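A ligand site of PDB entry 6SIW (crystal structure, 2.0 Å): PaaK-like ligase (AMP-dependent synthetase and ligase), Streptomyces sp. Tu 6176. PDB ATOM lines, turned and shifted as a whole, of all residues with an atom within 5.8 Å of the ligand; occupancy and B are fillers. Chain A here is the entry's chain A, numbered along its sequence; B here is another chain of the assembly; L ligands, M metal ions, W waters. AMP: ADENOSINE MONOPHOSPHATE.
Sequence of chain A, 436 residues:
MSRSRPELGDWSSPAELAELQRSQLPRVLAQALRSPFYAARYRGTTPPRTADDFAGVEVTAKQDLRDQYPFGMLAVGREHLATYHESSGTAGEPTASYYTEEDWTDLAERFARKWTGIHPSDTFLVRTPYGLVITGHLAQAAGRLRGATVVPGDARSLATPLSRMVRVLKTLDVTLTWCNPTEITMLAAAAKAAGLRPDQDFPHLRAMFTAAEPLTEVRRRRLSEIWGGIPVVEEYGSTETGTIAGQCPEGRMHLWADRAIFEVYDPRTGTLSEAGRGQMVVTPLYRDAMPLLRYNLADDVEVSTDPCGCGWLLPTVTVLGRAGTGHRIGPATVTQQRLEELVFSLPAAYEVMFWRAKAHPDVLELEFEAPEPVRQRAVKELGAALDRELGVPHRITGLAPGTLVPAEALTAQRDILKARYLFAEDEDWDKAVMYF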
ATOM      1  N   LYS A  62     -21.382  -9.064  -4.092  1.00  0.00           N
ATOM      2  CA  LYS A  62     -20.310  -8.758  -3.105  1.00  0.00           C
ATOM      3  C   LYS A  62     -20.491  -7.337  -2.585  1.00  0.00           C
ATOM      4  O   LYS A  62     -20.385  -7.127  -1.355  1.00  0.00           O
ATOM      5  CB  LYS A  62     -18.940  -8.862  -3.756  1.00  0.00           C
ATOM      6  CG  LYS A  62     -18.244 -10.207  -3.598  1.00  0.00           C
ATOM      7  CD  LYS A  62     -16.779 -10.050  -3.227  1.00  0.00           C
ATOM      8  CE  LYS A  62     -16.109 -11.367  -2.877  1.00  0.00           C
ATOM      9  NZ  LYS A  62     -16.240 -12.352  -3.971  1.00  0.00           N
ATOM     10  N   SER A  87     -13.837 -11.435   5.360  1.00  0.00           N
ATOM     11  CA  SER A  87     -13.267 -12.189   4.218  1.00  0.00           C
ATOM     12  C   SER A  87     -11.841 -11.696   3.976  1.00  0.00           C
ATOM     13  O   SER A  87     -11.531 -10.546   4.370  1.00  0.00           O
ATOM     14  CB  SER A  87     -14.121 -12.057   2.984  1.00  0.00           C
ATOM     15  OG  SER A  87     -15.391 -12.686   3.188  1.00  0.00           O
ATOM     16  N   SER A  88     -11.035 -12.517   3.299  1.00  0.00           N
ATOM     17  CA  SER A  88      -9.726 -12.096   2.730  1.00  0.00           C
ATOM     18  C   SER A  88      -9.977 -11.036   1.645  1.00  0.00           C
ATOM     19  O   SER A  88     -11.153 -10.674   1.381  1.00  0.00           O
ATOM     20  CB  SER A  88      -8.947 -13.298   2.268  1.00  0.00           C
ATOM     21  OG  SER A  88      -9.393 -13.748   1.005  1.00  0.00           O
ATOM     22  N   GLY A  89      -8.910 -10.485   1.061  1.00  0.00           N
ATOM     23  CA  GLY A  89      -9.006  -9.380   0.082  1.00  0.00           C
ATOM     24  C   GLY A  89      -8.908  -8.018   0.747  1.00  0.00           C
ATOM     25  O   GLY A  89      -8.307  -7.949   1.859  1.00  0.00           O
ATOM     26  N   VAL A 133     -10.593 -14.306   9.309  1.00  0.00           N
ATOM     27  CA  VAL A 133     -11.031 -15.275   8.265  1.00  0.00           C
ATOM     28  C   VAL A 133     -11.517 -16.560   8.934  1.00  0.00           C
ATOM     29  O   VAL A 133     -11.141 -16.845  10.087  1.00  0.00           O
ATOM     30  CB  VAL A 133      -9.946 -15.534   7.193  1.00  0.00           C
ATOM     31  CG1 VAL A 133      -9.666 -14.272   6.364  1.00  0.00           C
ATOM     32  CG2 VAL A 133      -8.668 -16.076   7.770  1.00  0.00           C
ATOM     33  N   THR A 135     -11.095 -19.721   7.704  1.00  0.00           N
ATOM     34  CA  THR A 135     -10.424 -20.937   7.195  1.00  0.00           C
ATOM     35  C   THR A 135      -9.835 -21.789   8.334  1.00  0.00           C
ATOM     36  O   THR A 135     -10.075 -22.983   8.316  1.00  0.00           O
ATOM     37  CB  THR A 135      -9.411 -20.626   6.097  1.00  0.00           C
ATOM     38  OG1 THR A 135      -8.758 -21.878   5.848  1.00  0.00           O
ATOM     39  CG2 THR A 135      -8.401 -19.567   6.481  1.00  0.00           C
ATOM     40  N   THR A 210      -6.431 -28.797   0.616  1.00  0.00           N
ATOM     41  CA  THR A 210      -6.029 -27.484   0.077  1.00  0.00           C
ATOM     42  C   THR A 210      -7.222 -26.794  -0.572  1.00  0.00           C
ATOM     43  O   THR A 210      -8.196 -27.469  -0.872  1.00  0.00           O
ATOM     44  CB  THR A 210      -4.825 -27.695  -0.857  1.00  0.00           C
ATOM     45  OG1 THR A 210      -4.097 -26.466  -0.856  1.00  0.00           O
ATOM     46  CG2 THR A 210      -5.208 -28.101  -2.260  1.00  0.00           C
ATOM     47  N   ALA A 211      -7.109 -25.491  -0.760  1.00  0.00           N
ATOM     48  CA  ALA A 211      -8.150 -24.571  -1.272  1.00  0.00           C
ATOM     49  C   ALA A 211      -7.529 -23.180  -1.436  1.00  0.00           C
ATOM     50  O   ALA A 211      -6.329 -23.078  -1.208  1.00  0.00           O
ATOM     51  CB  ALA A 211      -9.304 -24.530  -0.318  1.00  0.00           C
ATOM     52  N   ALA A 212      -8.329 -22.171  -1.768  1.00  0.00           N
ATOM     53  CA  ALA A 212      -8.024 -20.723  -1.635  1.00  0.00           C
ATOM     54  C   ALA A 212      -7.337 -20.152  -2.895  1.00  0.00           C
ATOM     55  O   ALA A 212      -7.282 -18.913  -2.978  1.00  0.00           O
ATOM     56  CB  ALA A 212      -7.183 -20.458  -0.403  1.00  0.00           C
ATOM     57  N   GLU A 213      -6.841 -20.975  -3.824  1.00  0.00           N
ATOM     58  CA  GLU A 213      -6.330 -20.446  -5.119  1.00  0.00           C
ATOM     59  C   GLU A 213      -6.607 -21.413  -6.271  1.00  0.00           C
ATOM     60  O   GLU A 213      -6.770 -22.612  -6.068  1.00  0.00           O
ATOM     61  CB  GLU A 213      -4.845 -20.039  -5.061  1.00  0.00           C
ATOM     62  CG  GLU A 213      -3.944 -21.005  -4.353  1.00  0.00           C
ATOM     63  CD  GLU A 213      -2.452 -20.722  -4.370  1.00  0.00           C
ATOM     64  OE1 GLU A 213      -1.846 -20.645  -3.259  1.00  0.00           O
ATOM     65  OE2 GLU A 213      -1.872 -20.720  -5.481  1.00  0.00           O
ATOM     66  N   PRO A 214      -6.723 -20.886  -7.502  1.00  0.00           N
ATOM     67  CA  PRO A 214      -6.890 -21.703  -8.698  1.00  0.00           C
ATOM     68  C   PRO A 214      -5.747 -22.705  -8.809  1.00  0.00           C
ATOM     69  O   PRO A 214      -4.608 -22.328  -8.696  1.00  0.00           O
ATOM     70  CB  PRO A 214      -6.817 -20.721  -9.860  1.00  0.00           C
ATOM     71  CG  PRO A 214      -7.216 -19.400  -9.245  1.00  0.00           C
ATOM     72  CD  PRO A 214      -6.722 -19.447  -7.825  1.00  0.00           C
ATOM     73  N   LEU A 215      -6.090 -23.966  -9.019  1.00  0.00           N
ATOM     74  CA  LEU A 215      -5.138 -25.099  -8.995  1.00  0.00           C
ATOM     75  C   LEU A 215      -5.442 -25.977 -10.198  1.00  0.00           C
ATOM     76  O   LEU A 215      -6.495 -26.610 -10.206  1.00  0.00           O
ATOM     77  CB  LEU A 215      -5.311 -25.836  -7.662  1.00  0.00           C
ATOM     78  CG  LEU A 215      -4.385 -27.022  -7.430  1.00  0.00           C
ATOM     79  CD1 LEU A 215      -2.947 -26.578  -7.388  1.00  0.00           C
ATOM     80  CD2 LEU A 215      -4.749 -27.747  -6.144  1.00  0.00           C
ATOM     81  N   GLU A 234      -8.673 -31.201  -2.814  1.00  0.00           N
ATOM     82  CA  GLU A 234      -9.011 -29.788  -3.038  1.00  0.00           C
ATOM     83  C   GLU A 234     -10.453 -29.552  -2.608  1.00  0.00           C
ATOM     84  O   GLU A 234     -11.311 -30.430  -2.859  1.00  0.00           O
ATOM     85  CB  GLU A 234      -8.819 -29.441  -4.502  1.00  0.00           C
ATOM     86  CG  GLU A 234      -8.925 -27.952  -4.774  1.00  0.00           C
ATOM     87  CD  GLU A 234      -8.841 -27.575  -6.235  1.00  0.00           C
ATOM     88  OE1 GLU A 234      -8.747 -28.498  -7.089  1.00  0.00           O
ATOM     89  OE2 GLU A 234      -8.859 -26.363  -6.506  1.00  0.00           O
ATOM     90  N   GLU A 235     -10.698 -28.398  -2.011  1.00  0.00           N
ATOM     91  CA  GLU A 235     -12.080 -27.903  -1.843  1.00  0.00           C
ATOM     92  C   GLU A 235     -12.117 -26.462  -2.342  1.00  0.00           C
ATOM     93  O   GLU A 235     -11.044 -25.870  -2.555  1.00  0.00           O
ATOM     94  CB  GLU A 235     -12.565 -28.092  -0.409  1.00  0.00           C
ATOM     95  CG  GLU A 235     -12.029 -27.065   0.565  1.00  0.00           C
ATOM     96  CD  GLU A 235     -12.851 -27.010   1.839  1.00  0.00           C
ATOM     97  OE1 GLU A 235     -13.070 -28.087   2.455  1.00  0.00           O
ATOM     98  OE2 GLU A 235     -13.330 -25.895   2.165  1.00  0.00           O
ATOM     99  N   TYR A 236     -13.327 -25.975  -2.551  1.00  0.00           N
ATOM    100  CA  TYR A 236     -13.671 -24.612  -3.000  1.00  0.00           C
ATOM    101  C   TYR A 236     -14.626 -24.045  -1.946  1.00  0.00           C
ATOM    102  O   TYR A 236     -15.614 -24.727  -1.622  1.00  0.00           O
ATOM    103  CB  TYR A 236     -14.277 -24.682  -4.389  1.00  0.00           C
ATOM    104  CG  TYR A 236     -14.900 -23.413  -4.917  1.00  0.00           C
ATOM    105  CD1 TYR A 236     -14.344 -22.169  -4.684  1.00  0.00           C
ATOM    106  CD2 TYR A 236     -15.985 -23.474  -5.763  1.00  0.00           C
ATOM    107  CE1 TYR A 236     -14.903 -21.010  -5.210  1.00  0.00           C
ATOM    108  CE2 TYR A 236     -16.557 -22.334  -6.308  1.00  0.00           C
ATOM    109  CZ  TYR A 236     -16.006 -21.092  -6.043  1.00  0.00           C
ATOM    110  OH  TYR A 236     -16.553 -19.970  -6.607  1.00  0.00           O
ATOM    111  N   GLY A 237     -14.272 -22.889  -1.377  1.00  0.00           N
ATOM    112  CA  GLY A 237     -15.125 -22.207  -0.389  1.00  0.00           C
ATOM    113  C   GLY A 237     -14.792 -20.736  -0.289  1.00  0.00           C
ATOM    114  O   GLY A 237     -13.966 -20.219  -1.073  1.00  0.00           O
ATOM    115  N   SER A 238     -15.442 -20.068   0.640  1.00  0.00           N
ATOM    116  CA  SER A 238     -15.262 -18.631   0.951  1.00  0.00           C
ATOM    117  C   SER A 238     -15.680 -18.445   2.392  1.00  0.00           C
ATOM    118  O   SER A 238     -16.432 -19.305   2.901  1.00  0.00           O
ATOM    119  CB  SER A 238     -16.051 -17.753   0.009  1.00  0.00           C
ATOM    120  OG  SER A 238     -17.427 -17.749   0.353  1.00  0.00           O
ATOM    121  N   THR A 239     -15.202 -17.386   3.030  1.00  0.00           N
ATOM    122  CA  THR A 239     -15.545 -17.030   4.421  1.00  0.00           C
ATOM    123  C   THR A 239     -17.069 -16.877   4.516  1.00  0.00           C
ATOM    124  O   THR A 239     -17.646 -17.365   5.503  1.00  0.00           O
ATOM    125  CB  THR A 239     -14.753 -15.785   4.852  1.00  0.00           C
ATOM    126  OG1 THR A 239     -13.365 -16.115   4.825  1.00  0.00           O
ATOM    127  CG2 THR A 239     -15.157 -15.292   6.210  1.00  0.00           C
ATOM    128  N   GLU A 240     -17.695 -16.248   3.523  1.00  0.00           N
ATOM    129  CA  GLU A 240     -19.115 -15.855   3.661  1.00  0.00           C
ATOM    130  C   GLU A 240     -20.045 -17.021   3.273  1.00  0.00           C
ATOM    131  O   GLU A 240     -21.252 -16.882   3.562  1.00  0.00           O
ATOM    132  CB  GLU A 240     -19.388 -14.559   2.882  1.00  0.00           C
ATOM    133  CG  GLU A 240     -19.071 -14.621   1.402  1.00  0.00           C
ATOM    134  CD  GLU A 240     -17.674 -14.164   0.999  1.00  0.00           C
ATOM    135  OE1 GLU A 240     -16.746 -14.247   1.841  1.00  0.00           O
ATOM    136  OE2 GLU A 240     -17.514 -13.757  -0.176  1.00  0.00           O
ATOM    137  N   MET A 253     -13.737 -31.619  -8.365  1.00  0.00           N
ATOM    138  CA  MET A 253     -14.508 -30.999  -7.255  1.00  0.00           C
ATOM    139  C   MET A 253     -15.996 -31.092  -7.611  1.00  0.00           C
ATOM    140  O   MET A 253     -16.380 -30.679  -8.735  1.00  0.00           O
ATOM    141  CB  MET A 253     -14.113 -29.538  -7.013  1.00  0.00           C
ATOM    142  CG  MET A 253     -12.728 -29.386  -6.421  1.00  0.00           C
ATOM    143  SD  MET A 253     -12.428 -27.725  -5.783  1.00  0.00           S
ATOM    144  CE  MET A 253     -12.371 -26.801  -7.314  1.00  0.00           C
ATOM    145  N   LEU A 297     -20.533 -14.955  -5.804  1.00  0.00           N
ATOM    146  CA  LEU A 297     -19.126 -15.011  -5.307  1.00  0.00           C
ATOM    147  C   LEU A 297     -18.224 -14.329  -6.359  1.00  0.00           C
ATOM    148  O   LEU A 297     -17.122 -13.897  -6.001  1.00  0.00           O
ATOM    149  CB  LEU A 297     -18.786 -16.482  -5.073  1.00  0.00           C
ATOM    150  CG  LEU A 297     -17.750 -16.836  -4.006  1.00  0.00           C
ATOM    151  CD1 LEU A 297     -17.853 -15.987  -2.744  1.00  0.00           C
ATOM    152  CD2 LEU A 297     -17.883 -18.307  -3.643  1.00  0.00           C
ATOM    153  N   ASP A 299     -16.587 -15.564  -8.751  1.00  0.00           N
ATOM    154  CA  ASP A 299     -15.499 -16.422  -9.291  1.00  0.00           C
ATOM    155  C   ASP A 299     -15.936 -16.901 -10.684  1.00  0.00           C
ATOM    156  O   ASP A 299     -17.118 -17.283 -10.840  1.00  0.00           O
ATOM    157  CB  ASP A 299     -15.181 -17.617  -8.393  1.00  0.00           C
ATOM    158  CG  ASP A 299     -14.590 -17.240  -7.052  1.00  0.00           C
ATOM    159  OD1 ASP A 299     -13.650 -16.406  -7.026  1.00  0.00           O
ATOM    160  OD2 ASP A 299     -15.092 -17.775  -6.016  1.00  0.00           O
ATOM    161  N   VAL A 319     -12.770 -24.076 -11.052  1.00  0.00           N
ATOM    162  CA  VAL A 319     -12.712 -22.658 -10.605  1.00  0.00           C
ATOM    163  C   VAL A 319     -11.490 -22.005 -11.280  1.00  0.00           C
ATOM    164  O   VAL A 319     -10.363 -22.326 -10.891  1.00  0.00           O
ATOM    165  CB  VAL A 319     -12.667 -22.533  -9.076  1.00  0.00           C
ATOM    166  CG1 VAL A 319     -12.807 -21.089  -8.618  1.00  0.00           C
ATOM    167  CG2 VAL A 319     -13.707 -23.403  -8.404  1.00  0.00           C
ATOM    168  N   LEU A 320     -11.731 -21.130 -12.252  1.00  0.00           N
ATOM    169  CA  LEU A 320     -10.681 -20.299 -12.908  1.00  0.00           C
ATOM    170  C   LEU A 320     -10.337 -19.118 -11.977  1.00  0.00           C
ATOM    171  O   LEU A 320      -9.140 -18.854 -11.775  1.00  0.00           O
ATOM    172  CB  LEU A 320     -11.205 -19.820 -14.259  1.00  0.00           C
ATOM    173  CG  LEU A 320     -11.496 -20.891 -15.313  1.00  0.00           C
ATOM    174  CD1 LEU A 320     -10.557 -22.073 -15.209  1.00  0.00           C
ATOM    175  CD2 LEU A 320     -12.950 -21.356 -15.264  1.00  0.00           C
ATOM    176  N   GLY A 321     -11.343 -18.435 -11.418  1.00  0.00           N
ATOM    177  CA  GLY A 321     -11.165 -17.141 -10.739  1.00  0.00           C
ATOM    178  C   GLY A 321     -10.386 -16.166 -11.621  1.00  0.00           C
ATOM    179  O   GLY A 321     -10.648 -16.160 -12.829  1.00  0.00           O
ATOM    180  N   LYS B 419      -3.989 -13.529  -1.416  1.00  0.00           N
ATOM    181  CA  LYS B 419      -3.674 -14.922  -1.800  1.00  0.00           C
ATOM    182  C   LYS B 419      -2.494 -14.875  -2.766  1.00  0.00           C
ATOM    183  O   LYS B 419      -2.236 -13.792  -3.352  1.00  0.00           O
ATOM    184  CB  LYS B 419      -4.897 -15.572  -2.454  1.00  0.00           C
ATOM    185  CG  LYS B 419      -6.175 -15.563  -1.634  1.00  0.00           C
ATOM    186  CD  LYS B 419      -6.084 -16.411  -0.362  1.00  0.00           C
ATOM    187  CE  LYS B 419      -7.388 -16.449   0.434  1.00  0.00           C
ATOM    188  NZ  LYS B 419      -8.539 -16.903  -0.390  1.00  0.00           N
HETATM  189  P   AMP L   1     -11.740 -16.486   1.376  1.00  0.00           P
HETATM  190  O1P AMP L   1     -13.034 -15.800   1.721  1.00  0.00           O
HETATM  191  O2P AMP L   1     -10.542 -15.748   1.916  1.00  0.00           O
HETATM  192  O3P AMP L   1     -11.709 -17.966   1.712  1.00  0.00           O
HETATM  193  O5' AMP L   1     -11.600 -16.443  -0.236  1.00  0.00           O
HETATM  194  C5' AMP L   1     -12.537 -17.190  -1.061  1.00  0.00           C
HETATM  195  C4' AMP L   1     -12.086 -17.109  -2.488  1.00  0.00           C
HETATM  196  O4' AMP L   1     -10.878 -17.893  -2.680  1.00  0.00           O
HETATM  197  C3' AMP L   1     -13.040 -17.677  -3.546  1.00  0.00           C
HETATM  198  O3' AMP L   1     -14.062 -16.747  -3.880  1.00  0.00           O
HETATM  199  C2' AMP L   1     -12.073 -17.893  -4.711  1.00  0.00           C
HETATM  200  O2' AMP L   1     -11.813 -16.689  -5.404  1.00  0.00           O
HETATM  201  C1' AMP L   1     -10.851 -18.433  -3.985  1.00  0.00           C
HETATM  202  N9  AMP L   1     -10.836 -19.892  -3.903  1.00  0.00           N
HETATM  203  C8  AMP L   1     -11.164 -20.664  -2.822  1.00  0.00           C
HETATM  204  N7  AMP L   1     -11.053 -21.953  -3.047  1.00  0.00           N
HETATM  205  C5  AMP L   1     -10.630 -22.026  -4.373  1.00  0.00           C
HETATM  206  C6  AMP L   1     -10.328 -23.117  -5.207  1.00  0.00           C
HETATM  207  N6  AMP L   1     -10.427 -24.394  -4.837  1.00  0.00           N
HETATM  208  N1  AMP L   1      -9.930 -22.844  -6.465  1.00  0.00           N
HETATM  209  C2  AMP L   1      -9.860 -21.562  -6.845  1.00  0.00           C
HETATM  210  N3  AMP L   1     -10.096 -20.466  -6.148  1.00  0.00           N
HETATM  211  C4  AMP L   1     -10.491 -20.766  -4.901  1.00  0.00           C
HETATM  212 MG    MG M   1     -14.497 -14.175   0.202  1.00  0.00          MG
HETATM  213  O   HOH W   1     -11.497 -17.979   5.083  1.00  0.00           O
HETATM  214  O   HOH W   2      -9.023 -24.650  -8.313  1.00  0.00           O
HETATM  215  O   HOH W   3      -9.905 -17.937  -7.243  1.00  0.00           O
HETATM  216  O   HOH W   4     -12.480 -19.989   3.276  1.00  0.00           O
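N of Ala 212 is in hydrogen-bond range of N7 of the ligand, 3.0 Å away. OG1 of Thr 239 lies within hydrogen-bond range of O1P of the ligand, at 3.1 Å. OE2 of Glu 234 sits at hydrogen-bond distance from N6 of the ligand (3.0 Å). An oxygen (O2') of the ligand sits at hydrogen-bond distance from the side-chain carboxylate (OD1) of Asp 299 (2.5 Å). The side-chain hydroxyl (OG) of Ser 88 is in hydrogen-bond range of an oxygen (O2P) of the ligand, at 2.5 Å. O2P of the ligand lies within salt-bridge range of NZ of Lys 419 of chain B (3.3 Å). The backbone NH of Thr 239 sits at hydrogen-bond distance from an oxygen (O1P) of the ligand. The backbone carbonyl oxygen (O) of Glu 235 sits at hydrogen-bond distance from a nitrogen (N6) of the ligand.
The backbone carbonyl oxygen (O) of Leu 297 lies within hydrogen-bond range of the side-chain amino group (NZ) of Lys 62. The side-chain hydroxyl of Tyr 236 lies within hydrogen-bond range of the side-chain carboxylate of Asp 299, at 2.7 Å. The side-chain sulfur of Met 253 lies within hydrogen-bond range of the backbone NH of Tyr 236, at 3.8 Å. The backbone NH (N) of Glu 235 sits at hydrogen-bond distance from the backbone carbonyl oxygen (O) of Thr 210 (2.9 Å).
A nitrogen (N1) of the ligand lies close to the backbone carbonyl oxygen of Glu 213 (3.2 Å). Merely in contact with the ligand: Pro 214 (3.3 Å), Gly 237 (3.3 Å), Val 319 (3.5 Å), Ser 238 (3.7 Å), Tyr 236 (3.7 Å), Leu 297 (3.7 Å) and Met 253 (3.96 Å). Hydrophobic or aromatic side chains within 4 Å of the ligand: Pro 214, Tyr 236, Met 253, Leu 297 and Val 319.
Water W2 lies within hydrogen-bond range of OE2 of Glu 234, N1 of the ligand and N of Leu 215. Water W1 lies within hydrogen-bond range of the side-chain hydroxyl of Thr 239, the backbone NH of Thr 135 and an oxygen (O3P) of the ligand.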
